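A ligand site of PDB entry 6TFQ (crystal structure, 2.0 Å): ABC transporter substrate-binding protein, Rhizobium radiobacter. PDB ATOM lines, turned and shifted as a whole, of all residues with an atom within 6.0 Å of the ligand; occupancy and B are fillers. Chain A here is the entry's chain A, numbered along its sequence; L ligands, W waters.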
ATOM      1  N   THR A  24      12.000 -13.065  13.903  1.00  0.00           N
ATOM      2  CA  THR A  24      10.989 -14.105  13.697  1.00  0.00           C
ATOM      3  C   THR A  24      10.882 -15.089  14.842  1.00  0.00           C
ATOM      4  O   THR A  24       9.778 -15.498  15.183  1.00  0.00           O
ATOM      5  CB  THR A  24      11.268 -14.814  12.349  1.00  0.00           C
ATOM      6  OG1 THR A  24      11.180 -13.848  11.299  1.00  0.00           O
ATOM      7  CG2 THR A  24      10.297 -15.970  12.062  1.00  0.00           C
ATOM      8  N   THR A  25      12.010 -15.540  15.400  1.00  0.00           N
ATOM      9  CA  THR A  25      11.983 -16.493  16.506  1.00  0.00           C
ATOM     10  C   THR A  25      11.358 -15.788  17.702  1.00  0.00           C
ATOM     11  O   THR A  25      11.510 -14.569  17.826  1.00  0.00           O
ATOM     12  CB  THR A  25      13.394 -17.031  16.869  1.00  0.00           C
ATOM     13  OG1 THR A  25      14.186 -15.977  17.445  1.00  0.00           O
ATOM     14  CG2 THR A  25      14.129 -17.692  15.685  1.00  0.00           C
ATOM     15  N   THR A  26      10.677 -16.540  18.574  1.00  0.00           N
ATOM     16  CA  THR A  26      10.084 -15.975  19.793  1.00  0.00           C
ATOM     17  C   THR A  26      11.079 -15.102  20.556  1.00  0.00           C
ATOM     18  O   THR A  26      10.733 -13.976  20.917  1.00  0.00           O
ATOM     19  CB  THR A  26       9.493 -17.088  20.679  1.00  0.00           C
ATOM     20  OG1 THR A  26       8.356 -17.611  20.000  1.00  0.00           O
ATOM     21  CG2 THR A  26       9.053 -16.561  22.078  1.00  0.00           C
ATOM     22  N   SER A  27      12.305 -15.608  20.776  1.00  0.00           N
ATOM     23  CA  SER A  27      13.362 -14.896  21.488  1.00  0.00           C
ATOM     24  C   SER A  27      13.734 -13.544  20.858  1.00  0.00           C
ATOM     25  O   SER A  27      13.781 -12.547  21.581  1.00  0.00           O
ATOM     26  CB  SER A  27      14.589 -15.779  21.672  1.00  0.00           C
ATOM     27  OG  SER A  27      15.526 -15.167  22.549  1.00  0.00           O
ATOM     28  N   ARG A  29      11.866 -11.753  18.722  1.00  0.00           N
ATOM     29  CA  ARG A  29      10.629 -10.963  18.802  1.00  0.00           C
ATOM     30  C   ARG A  29      10.428 -10.400  20.192  1.00  0.00           C
ATOM     31  O   ARG A  29       9.975  -9.264  20.316  1.00  0.00           O
ATOM     32  CB  ARG A  29       9.409 -11.802  18.387  1.00  0.00           C
ATOM     33  CG  ARG A  29       9.347 -12.140  16.901  1.00  0.00           C
ATOM     34  CD  ARG A  29       8.048 -12.891  16.677  1.00  0.00           C
ATOM     35  NE  ARG A  29       7.900 -13.451  15.340  1.00  0.00           N
ATOM     36  CZ  ARG A  29       7.309 -12.838  14.319  1.00  0.00           C
ATOM     37  NH1 ARG A  29       6.863 -11.593  14.444  1.00  0.00           N
ATOM     38  NH2 ARG A  29       7.180 -13.451  13.156  1.00  0.00           N
ATOM     39  N   PHE A 142       4.284  -5.186  16.620  1.00  0.00           N
ATOM     40  CA  PHE A 142       4.513  -6.585  16.272  1.00  0.00           C
ATOM     41  C   PHE A 142       4.999  -6.646  14.836  1.00  0.00           C
ATOM     42  O   PHE A 142       4.616  -5.795  14.044  1.00  0.00           O
ATOM     43  CB  PHE A 142       3.255  -7.482  16.488  1.00  0.00           C
ATOM     44  CG  PHE A 142       3.541  -8.972  16.432  1.00  0.00           C
ATOM     45  CD1 PHE A 142       4.417  -9.569  17.346  1.00  0.00           C
ATOM     46  CD2 PHE A 142       2.941  -9.773  15.471  1.00  0.00           C
ATOM     47  CE1 PHE A 142       4.668 -10.942  17.292  1.00  0.00           C
ATOM     48  CE2 PHE A 142       3.194 -11.150  15.427  1.00  0.00           C
ATOM     49  CZ  PHE A 142       4.057 -11.725  16.341  1.00  0.00           C
ATOM     50  N   GLN A 223      11.241 -19.143  31.026  1.00  0.00           N
ATOM     51  CA  GLN A 223      10.291 -19.689  30.069  1.00  0.00           C
ATOM     52  C   GLN A 223       9.997 -21.129  30.509  1.00  0.00           C
ATOM     53  O   GLN A 223      10.896 -21.818  30.989  1.00  0.00           O
ATOM     54  CB  GLN A 223      10.883 -19.666  28.654  1.00  0.00           C
ATOM     55  CG  GLN A 223       9.887 -20.101  27.588  1.00  0.00           C
ATOM     56  CD  GLN A 223      10.381 -19.861  26.189  1.00  0.00           C
ATOM     57  OE1 GLN A 223      11.427 -19.233  25.966  1.00  0.00           O
ATOM     58  NE2 GLN A 223       9.639 -20.302  25.214  1.00  0.00           N
ATOM     59  N   GLN A 226       5.241 -26.893  27.477  1.00  0.00           N
ATOM     60  CA  GLN A 226       3.791 -27.158  27.274  1.00  0.00           C
ATOM     61  C   GLN A 226       3.271 -28.308  28.126  1.00  0.00           C
ATOM     62  O   GLN A 226       2.104 -28.670  28.001  1.00  0.00           O
ATOM     63  CB  GLN A 226       3.481 -27.399  25.789  1.00  0.00           C
ATOM     64  CG  GLN A 226       3.778 -26.192  24.881  1.00  0.00           C
ATOM     65  CD  GLN A 226       5.266 -25.918  24.690  1.00  0.00           C
ATOM     66  OE1 GLN A 226       6.065 -26.819  24.391  1.00  0.00           O
ATOM     67  NE2 GLN A 226       5.664 -24.683  24.883  1.00  0.00           N
ATOM     68  N   GLU A 249      -0.087 -20.552  20.255  1.00  0.00           N
ATOM     69  CA  GLU A 249       0.607 -20.785  18.986  1.00  0.00           C
ATOM     70  C   GLU A 249       0.173 -22.122  18.424  1.00  0.00           C
ATOM     71  O   GLU A 249       0.291 -23.137  19.112  1.00  0.00           O
ATOM     72  CB  GLU A 249       2.131 -20.732  19.159  1.00  0.00           C
ATOM     73  CG  GLU A 249       2.647 -19.388  19.615  1.00  0.00           C
ATOM     74  CD  GLU A 249       4.151 -19.380  19.763  1.00  0.00           C
ATOM     75  OE1 GLU A 249       4.636 -19.839  20.819  1.00  0.00           O
ATOM     76  OE2 GLU A 249       4.840 -18.929  18.829  1.00  0.00           O
ATOM     77  N   LEU A 250      -0.350 -22.111  17.187  1.00  0.00           N
ATOM     78  CA  LEU A 250      -0.761 -23.354  16.538  1.00  0.00           C
ATOM     79  C   LEU A 250       0.407 -24.076  15.869  1.00  0.00           C
ATOM     80  O   LEU A 250       1.156 -23.489  15.078  1.00  0.00           O
ATOM     81  CB  LEU A 250      -1.917 -23.113  15.530  1.00  0.00           C
ATOM     82  CG  LEU A 250      -2.371 -24.308  14.689  1.00  0.00           C
ATOM     83  CD1 LEU A 250      -2.952 -25.452  15.548  1.00  0.00           C
ATOM     84  CD2 LEU A 250      -3.366 -23.889  13.618  1.00  0.00           C
ATOM     85  N   ASN A 251       0.520 -25.371  16.172  1.00  0.00           N
ATOM     86  CA  ASN A 251       1.507 -26.272  15.616  1.00  0.00           C
ATOM     87  C   ASN A 251       0.864 -27.093  14.523  1.00  0.00           C
ATOM     88  O   ASN A 251      -0.200 -27.665  14.740  1.00  0.00           O
ATOM     89  CB  ASN A 251       2.057 -27.204  16.689  1.00  0.00           C
ATOM     90  CG  ASN A 251       2.634 -26.484  17.856  1.00  0.00           C
ATOM     91  OD1 ASN A 251       3.667 -25.830  17.747  1.00  0.00           O
ATOM     92  ND2 ASN A 251       2.000 -26.584  18.992  1.00  0.00           N
ATOM     93  N   ARG A 284      -0.276 -33.462  27.084  1.00  0.00           N
ATOM     94  CA  ARG A 284       0.364 -32.207  27.483  1.00  0.00           C
ATOM     95  C   ARG A 284      -0.388 -31.439  28.593  1.00  0.00           C
ATOM     96  O   ARG A 284       0.264 -30.901  29.486  1.00  0.00           O
ATOM     97  CB  ARG A 284       0.603 -31.316  26.266  1.00  0.00           C
ATOM     98  CG  ARG A 284       1.748 -31.824  25.404  1.00  0.00           C
ATOM     99  CD  ARG A 284       2.079 -30.880  24.276  1.00  0.00           C
ATOM    100  NE  ARG A 284       3.505 -30.989  23.982  1.00  0.00           N
ATOM    101  CZ  ARG A 284       4.179 -30.210  23.146  1.00  0.00           C
ATOM    102  NH1 ARG A 284       3.561 -29.246  22.492  1.00  0.00           N
ATOM    103  NH2 ARG A 284       5.474 -30.391  22.976  1.00  0.00           N
ATOM    104  N   LEU A 339      14.348 -26.442  19.503  1.00  0.00           N
ATOM    105  CA  LEU A 339      13.565 -25.653  20.463  1.00  0.00           C
ATOM    106  C   LEU A 339      12.861 -26.785  21.279  1.00  0.00           C
ATOM    107  O   LEU A 339      12.289 -27.666  20.633  1.00  0.00           O
ATOM    108  CB  LEU A 339      12.509 -24.778  19.767  1.00  0.00           C
ATOM    109  CG  LEU A 339      11.578 -23.997  20.703  1.00  0.00           C
ATOM    110  CD1 LEU A 339      12.357 -22.936  21.486  1.00  0.00           C
ATOM    111  CD2 LEU A 339      10.368 -23.407  19.968  1.00  0.00           C
ATOM    112  N   PRO A 340      13.046 -26.883  22.628  1.00  0.00           N
ATOM    113  CA  PRO A 340      12.569 -28.083  23.349  1.00  0.00           C
ATOM    114  C   PRO A 340      11.086 -28.450  23.176  1.00  0.00           C
ATOM    115  O   PRO A 340      10.810 -29.646  23.059  1.00  0.00           O
ATOM    116  CB  PRO A 340      12.942 -27.807  24.811  1.00  0.00           C
ATOM    117  CG  PRO A 340      14.134 -26.882  24.701  1.00  0.00           C
ATOM    118  CD  PRO A 340      13.798 -25.987  23.537  1.00  0.00           C
ATOM    119  N   GLY A 341      10.192 -27.462  23.090  1.00  0.00           N
ATOM    120  CA  GLY A 341       8.776 -27.705  22.865  1.00  0.00           C
ATOM    121  C   GLY A 341       8.501 -28.342  21.515  1.00  0.00           C
ATOM    122  O   GLY A 341       7.693 -29.262  21.433  1.00  0.00           O
ATOM    123  N   LEU A 342       9.195 -27.878  20.452  1.00  0.00           N
ATOM    124  CA  LEU A 342       9.063 -28.432  19.102  1.00  0.00           C
ATOM    125  C   LEU A 342       9.695 -29.834  19.033  1.00  0.00           C
ATOM    126  O   LEU A 342       9.186 -30.714  18.338  1.00  0.00           O
ATOM    127  CB  LEU A 342       9.674 -27.501  18.034  1.00  0.00           C
ATOM    128  CG  LEU A 342       8.825 -26.262  17.653  1.00  0.00           C
ATOM    129  CD1 LEU A 342       9.602 -25.306  16.723  1.00  0.00           C
ATOM    130  CD2 LEU A 342       7.482 -26.654  17.002  1.00  0.00           C
ATOM    131  N   LEU A 345       7.331 -32.297  20.791  1.00  0.00           N
ATOM    132  CA  LEU A 345       6.166 -32.480  19.929  1.00  0.00           C
ATOM    133  C   LEU A 345       6.472 -33.435  18.771  1.00  0.00           C
ATOM    134  O   LEU A 345       5.689 -34.358  18.548  1.00  0.00           O
ATOM    135  CB  LEU A 345       5.620 -31.132  19.432  1.00  0.00           C
ATOM    136  CG  LEU A 345       4.310 -31.166  18.612  1.00  0.00           C
ATOM    137  CD1 LEU A 345       3.163 -31.957  19.325  1.00  0.00           C
ATOM    138  CD2 LEU A 345       3.874 -29.763  18.301  1.00  0.00           C
ATOM    139  N   HIS A 367      17.377 -24.345  16.503  1.00  0.00           N
ATOM    140  CA  HIS A 367      16.173 -23.597  16.134  1.00  0.00           C
ATOM    141  C   HIS A 367      16.352 -22.500  15.064  1.00  0.00           C
ATOM    142  O   HIS A 367      15.632 -22.523  14.060  1.00  0.00           O
ATOM    143  CB  HIS A 367      15.518 -23.025  17.405  1.00  0.00           C
ATOM    144  CG  HIS A 367      14.175 -22.413  17.179  1.00  0.00           C
ATOM    145  ND1 HIS A 367      13.117 -23.148  16.669  1.00  0.00           N
ATOM    146  CD2 HIS A 367      13.751 -21.149  17.440  1.00  0.00           C
ATOM    147  CE1 HIS A 367      12.084 -22.320  16.660  1.00  0.00           C
ATOM    148  NE2 HIS A 367      12.430 -21.108  17.100  1.00  0.00           N
ATOM    149  N   TRP A 370      17.623 -24.039  11.819  1.00  0.00           N
ATOM    150  CA  TRP A 370      16.463 -24.770  11.314  1.00  0.00           C
ATOM    151  C   TRP A 370      15.489 -23.804  10.569  1.00  0.00           C
ATOM    152  O   TRP A 370      14.984 -24.158   9.496  1.00  0.00           O
ATOM    153  CB  TRP A 370      15.760 -25.484  12.474  1.00  0.00           C
ATOM    154  CG  TRP A 370      14.425 -26.079  12.113  1.00  0.00           C
ATOM    155  CD1 TRP A 370      14.195 -27.269  11.486  1.00  0.00           C
ATOM    156  CD2 TRP A 370      13.141 -25.508  12.390  1.00  0.00           C
ATOM    157  NE1 TRP A 370      12.851 -27.496  11.384  1.00  0.00           N
ATOM    158  CE2 TRP A 370      12.168 -26.423  11.927  1.00  0.00           C
ATOM    159  CE3 TRP A 370      12.703 -24.315  13.013  1.00  0.00           C
ATOM    160  CZ2 TRP A 370      10.790 -26.201  12.068  1.00  0.00           C
ATOM    161  CZ3 TRP A 370      11.338 -24.096  13.161  1.00  0.00           C
ATOM    162  CH2 TRP A 370      10.397 -25.030  12.694  1.00  0.00           C
ATOM    163  N   HIS A 371      15.244 -22.592  11.143  1.00  0.00           N
ATOM    164  CA  HIS A 371      14.391 -21.563  10.540  1.00  0.00           C
ATOM    165  C   HIS A 371      14.855 -21.220   9.103  1.00  0.00           C
ATOM    166  O   HIS A 371      14.004 -21.066   8.230  1.00  0.00           O
ATOM    167  CB  HIS A 371      14.310 -20.300  11.418  1.00  0.00           C
ATOM    168  CG  HIS A 371      13.128 -20.287  12.335  1.00  0.00           C
ATOM    169  ND1 HIS A 371      11.890 -19.841  11.902  1.00  0.00           N
ATOM    170  CD2 HIS A 371      13.020 -20.669  13.625  1.00  0.00           C
ATOM    171  CE1 HIS A 371      11.094 -19.941  12.945  1.00  0.00           C
ATOM    172  NE2 HIS A 371      11.726 -20.443  13.992  1.00  0.00           N
ATOM    173  N   ARG A 375      13.234 -22.626   5.084  1.00  0.00           N
ATOM    174  CA  ARG A 375      13.033 -21.545   4.111  1.00  0.00           C
ATOM    175  C   ARG A 375      13.883 -21.743   2.829  1.00  0.00           C
ATOM    176  O   ARG A 375      13.861 -20.887   1.939  1.00  0.00           O
ATOM    177  CB  ARG A 375      13.252 -20.151   4.770  1.00  0.00           C
ATOM    178  CG  ARG A 375      12.066 -19.712   5.636  1.00  0.00           C
ATOM    179  CD  ARG A 375      12.446 -18.551   6.547  1.00  0.00           C
ATOM    180  NE  ARG A 375      11.339 -18.062   7.381  1.00  0.00           N
ATOM    181  CZ  ARG A 375      10.949 -18.587   8.545  1.00  0.00           C
ATOM    182  NH1 ARG A 375      11.532 -19.678   9.031  1.00  0.00           N
ATOM    183  NH2 ARG A 375       9.960 -18.029   9.234  1.00  0.00           N
ATOM    184  N   TYR A 384       5.895 -26.647  12.350  1.00  0.00           N
ATOM    185  CA  TYR A 384       5.988 -25.226  12.684  1.00  0.00           C
ATOM    186  C   TYR A 384       4.895 -24.831  13.686  1.00  0.00           C
ATOM    187  O   TYR A 384       3.743 -25.216  13.514  1.00  0.00           O
ATOM    188  CB  TYR A 384       5.864 -24.407  11.392  1.00  0.00           C
ATOM    189  CG  TYR A 384       6.539 -23.055  11.444  1.00  0.00           C
ATOM    190  CD1 TYR A 384       7.876 -22.899  11.084  1.00  0.00           C
ATOM    191  CD2 TYR A 384       5.817 -21.915  11.781  1.00  0.00           C
ATOM    192  CE1 TYR A 384       8.479 -21.641  11.070  1.00  0.00           C
ATOM    193  CE2 TYR A 384       6.410 -20.649  11.772  1.00  0.00           C
ATOM    194  CZ  TYR A 384       7.741 -20.516  11.415  1.00  0.00           C
ATOM    195  OH  TYR A 384       8.337 -19.282  11.403  1.00  0.00           O
ATOM    196  N   GLY A 385       5.263 -24.021  14.674  1.00  0.00           N
ATOM    197  CA  GLY A 385       4.348 -23.497  15.676  1.00  0.00           C
ATOM    198  C   GLY A 385       4.357 -21.993  15.733  1.00  0.00           C
ATOM    199  O   GLY A 385       5.393 -21.395  15.979  1.00  0.00           O
ATOM    200  N   ALA A 386       3.207 -21.351  15.462  1.00  0.00           N
ATOM    201  CA  ALA A 386       3.089 -19.894  15.463  1.00  0.00           C
ATOM    202  C   ALA A 386       1.667 -19.368  15.576  1.00  0.00           C
ATOM    203  O   ALA A 386       0.703 -20.063  15.261  1.00  0.00           O
ATOM    204  CB  ALA A 386       3.756 -19.290  14.198  1.00  0.00           C
ATOM    205  N   ALA A 387       1.560 -18.103  15.994  1.00  0.00           N
ATOM    206  CA  ALA A 387       0.316 -17.334  16.022  1.00  0.00           C
ATOM    207  C   ALA A 387       0.598 -16.086  15.169  1.00  0.00           C
ATOM    208  O   ALA A 387       1.758 -15.698  15.006  1.00  0.00           O
ATOM    209  CB  ALA A 387      -0.042 -16.926  17.451  1.00  0.00           C
ATOM    210  N   ARG A 388      -0.445 -15.492  14.618  1.00  0.00           N
ATOM    211  CA  ARG A 388      -0.359 -14.245  13.868  1.00  0.00           C
ATOM    212  C   ARG A 388      -1.434 -13.321  14.410  1.00  0.00           C
ATOM    213  O   ARG A 388      -2.199 -13.730  15.291  1.00  0.00           O
ATOM    214  CB  ARG A 388      -0.494 -14.463  12.350  1.00  0.00           C
ATOM    215  CG  ARG A 388       0.744 -15.085  11.684  1.00  0.00           C
ATOM    216  CD  ARG A 388       1.994 -14.227  11.832  1.00  0.00           C
ATOM    217  NE  ARG A 388       3.187 -14.821  11.222  1.00  0.00           N
ATOM    218  CZ  ARG A 388       4.136 -15.477  11.881  1.00  0.00           C
ATOM    219  NH1 ARG A 388       4.039 -15.671  13.192  1.00  0.00           N
ATOM    220  NH2 ARG A 388       5.193 -15.943  11.237  1.00  0.00           N
ATOM    221  N   PHE A 399       0.911 -18.719   5.382  1.00  0.00           N
ATOM    222  CA  PHE A 399       1.118 -20.150   5.382  1.00  0.00           C
ATOM    223  C   PHE A 399       0.552 -20.906   4.198  1.00  0.00           C
ATOM    224  O   PHE A 399       1.045 -22.002   3.935  1.00  0.00           O
ATOM    225  CB  PHE A 399       0.551 -20.766   6.684  1.00  0.00           C
ATOM    226  CG  PHE A 399       1.359 -20.440   7.928  1.00  0.00           C
ATOM    227  CD1 PHE A 399       2.437 -21.231   8.309  1.00  0.00           C
ATOM    228  CD2 PHE A 399       1.041 -19.328   8.699  1.00  0.00           C
ATOM    229  CE1 PHE A 399       3.171 -20.936   9.468  1.00  0.00           C
ATOM    230  CE2 PHE A 399       1.783 -19.028   9.847  1.00  0.00           C
ATOM    231  CZ  PHE A 399       2.815 -19.848  10.239  1.00  0.00           C
ATOM    232  N   VAL A 413       5.875 -18.293   4.853  1.00  0.00           N
ATOM    233  CA  VAL A 413       5.963 -19.558   5.587  1.00  0.00           C
ATOM    234  C   VAL A 413       5.064 -20.651   4.964  1.00  0.00           C
ATOM    235  O   VAL A 413       4.596 -21.557   5.662  1.00  0.00           O
ATOM    236  CB  VAL A 413       5.709 -19.339   7.111  1.00  0.00           C
ATOM    237  CG1 VAL A 413       6.959 -18.805   7.800  1.00  0.00           C
ATOM    238  CG2 VAL A 413       4.527 -18.412   7.358  1.00  0.00           C
ATOM    239  N   ASN A 460      -0.756 -23.912  21.677  1.00  0.00           N
ATOM    240  CA  ASN A 460      -0.323 -23.730  23.062  1.00  0.00           C
ATOM    241  C   ASN A 460      -0.189 -22.292  23.461  1.00  0.00           C
ATOM    242  O   ASN A 460       0.458 -21.507  22.757  1.00  0.00           O
ATOM    243  CB  ASN A 460       1.014 -24.445  23.346  1.00  0.00           C
ATOM    244  CG  ASN A 460       1.967 -24.564  22.172  1.00  0.00           C
ATOM    245  OD1 ASN A 460       2.087 -25.632  21.579  1.00  0.00           O
ATOM    246  ND2 ASN A 460       2.680 -23.502  21.792  1.00  0.00           N
ATOM    247  N   PRO A 481       4.090 -11.833  20.952  1.00  0.00           N
ATOM    248  CA  PRO A 481       5.046 -12.950  20.791  1.00  0.00           C
ATOM    249  C   PRO A 481       4.801 -14.191  21.682  1.00  0.00           C
ATOM    250  O   PRO A 481       5.520 -15.187  21.541  1.00  0.00           O
ATOM    251  CB  PRO A 481       6.415 -12.299  21.100  1.00  0.00           C
ATOM    252  CG  PRO A 481       6.169 -10.823  21.196  1.00  0.00           C
ATOM    253  CD  PRO A 481       4.741 -10.707  21.649  1.00  0.00           C
HETATM  254  O1  LIG L   1       5.406 -27.203  21.717  1.00  0.00           O
HETATM  255  C1  LIG L   1       5.399 -26.468  20.506  1.00  0.00           C
HETATM  256  C2  LIG L   1       6.395 -25.293  20.449  1.00  0.00           C
HETATM  257  O2  LIG L   1       7.022 -25.082  21.688  1.00  0.00           O
HETATM  258  C3  LIG L   1       5.805 -24.114  19.657  1.00  0.00           C
HETATM  259  O3  LIG L   1       4.416 -24.037  19.528  1.00  0.00           O
HETATM  260  C4  LIG L   1       6.093 -22.631  19.870  1.00  0.00           C
HETATM  261  O4  LIG L   1       6.481 -22.383  21.172  1.00  0.00           O
HETATM  262  C5  LIG L   1       7.030 -22.061  18.815  1.00  0.00           C
HETATM  263  O5  LIG L   1       7.049 -22.600  17.725  1.00  0.00           O
HETATM  264  C6  LIG L   1       7.826 -20.765  19.036  1.00  0.00           C
HETATM  265  N1  LIG L   1       7.262 -19.754  18.156  1.00  0.00           N
HETATM  266  C7  LIG L   1       8.080 -19.111  17.171  1.00  0.00           C
HETATM  267  C8  LIG L   1       9.389 -19.796  16.784  1.00  0.00           C
HETATM  268  O6  LIG L   1      10.390 -19.340  17.401  1.00  0.00           O
HETATM  269  C9  LIG L   1       7.188 -18.696  15.995  1.00  0.00           C
HETATM  270  C10 LIG L   1       7.879 -18.214  14.717  1.00  0.00           C
HETATM  271  C11 LIG L   1       7.165 -17.139  13.900  1.00  0.00           C
HETATM  272  O7  LIG L   1       6.641 -16.121  14.437  1.00  0.00           O
HETATM  273  O8  LIG L   1       7.133 -17.268  12.662  1.00  0.00           O
HETATM  274  O9  LIG L   1       9.556 -20.712  15.898  1.00  0.00           O
HETATM  275  O   HOH W   1       8.475 -23.113  23.193  1.00  0.00           O
HETATM  276  O   HOH W   2       5.673 -15.148  16.833  1.00  0.00           O
HETATM  277  O   HOH W   3       6.852 -19.046  22.074  1.00  0.00           O
HETATM  278  O   HOH W   4       8.110 -22.681  14.593  1.00  0.00           O
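The backbone carbonyl oxygen (O) of Thr 24 sits close to an oxygen (O7) of the ligand. Thr 25 touches the ligand (CA to O6, 3.4 Å). CD2 of Leu 339 touches C5 of the ligand, 3.8 Å away. Leu 342 touches the ligand. CB of Ala 386 touches C9 of the ligand (3.9 Å). Hydrophobic or aromatic side chains that line the ligand: Leu 339, Leu 342, His 367, His 371, Tyr 384 and Ala 386. Within 4 Å of the ligand: Thr 24, Thr 25, Thr 26, Arg 29, Gln 226, Glu 249, Asn 251, Arg 284, Leu 339, Gly 341, Leu 342, His 367, His 371, Tyr 384, Gly 385, Ala 386, Arg 388 and Asn 460.
ND2 of Asn 251 sits at hydrogen-bond distance from OD1 of Asn 460 (2.8 Å). The backbone carbonyl oxygen (O) of Asn 460 is in hydrogen-bond range of the backbone NH (N) of Glu 249 (2.7 Å). The side-chain hydroxyl (OH) of Tyr 384 lies within hydrogen-bond range of the guanidinium group (NH2) of Arg 375, at 3.0 Å. A ring nitrogen (NE2) of His 371 sits at hydrogen-bond distance from a ring nitrogen (NE2) of His 367. The backbone carbonyl oxygen (O) of Gly 341 lies within hydrogen-bond range of the guanidinium group (NH2) of Arg 284 (2.9 Å). A ring nitrogen (ND1) of His 371 is in hydrogen-bond range of the guanidinium group (NH1) of Arg 375 (2.9 Å). NE of Arg 29 lies within hydrogen-bond range of O of Thr 24 (2.8 Å). The backbone NH (N) of Ala 386 lies within hydrogen-bond range of the backbone carbonyl oxygen (O) of Leu 250.
Water W2 lies within hydrogen-bond range of O7 of the ligand (2.8 Å) and NE of Arg 29 (3.2 Å). Water W4 bridges an oxygen (O9) of the ligand and the backbone NH (N) of Gly 385. Water W3 lies within hydrogen-bond range of OE1 of Glu 249, OG1 of Thr 26 and O4 of the ligand.
OD1 of Asn 251 sits at hydrogen-bond distance from O3 of the ligand, at 2.6 Å. A nitrogen (N1) of the ligand is in salt-bridge range of the side-chain carboxylate (OE2) of Glu 249 (2.6 Å). The side-chain hydroxyl (OH) of Tyr 384 is in hydrogen-bond range of an oxygen (O8) of the ligand (2.7 Å). A nitrogen (N1) of the ligand sits close to the backbone carbonyl oxygen of Gly 385, at 3.3 Å. An oxygen (O6) of the ligand is in hydrogen-bond range of a ring nitrogen (NE2) of His 367, 2.7 Å away. The guanidinium group of Arg 388 lies within salt-bridge range of an oxygen (O8) of the ligand (2.7 Å). An oxygen (O1) of the ligand is in hydrogen-bond range of the side-chain amide oxygen of Gln 226, 2.8 Å away. An oxygen (O1) of the ligand is in hydrogen-bond range of the guanidinium group (NH1) of Arg 284. An oxygen (O9) of the ligand is in hydrogen-bond range of a ring nitrogen (NE2) of His 371, at 2.9 Å. ND2 of Asn 460 lies within hydrogen-bond range of O3 of the ligand (2.9 Å). O7 of the ligand lies within salt-bridge range of NH2 of Arg 29 (3.0 Å). O6 of the ligand is in hydrogen-bond range of N of Thr 26 (3.0 Å). A nitrogen (N1) of the ligand lies within hydrogen-bond range of the side-chain hydroxyl (OG1) of Thr 26, at 3.0 Å. O1 of the ligand lies within hydrogen-bond range of O of Gly 341, at 3.1 Å.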
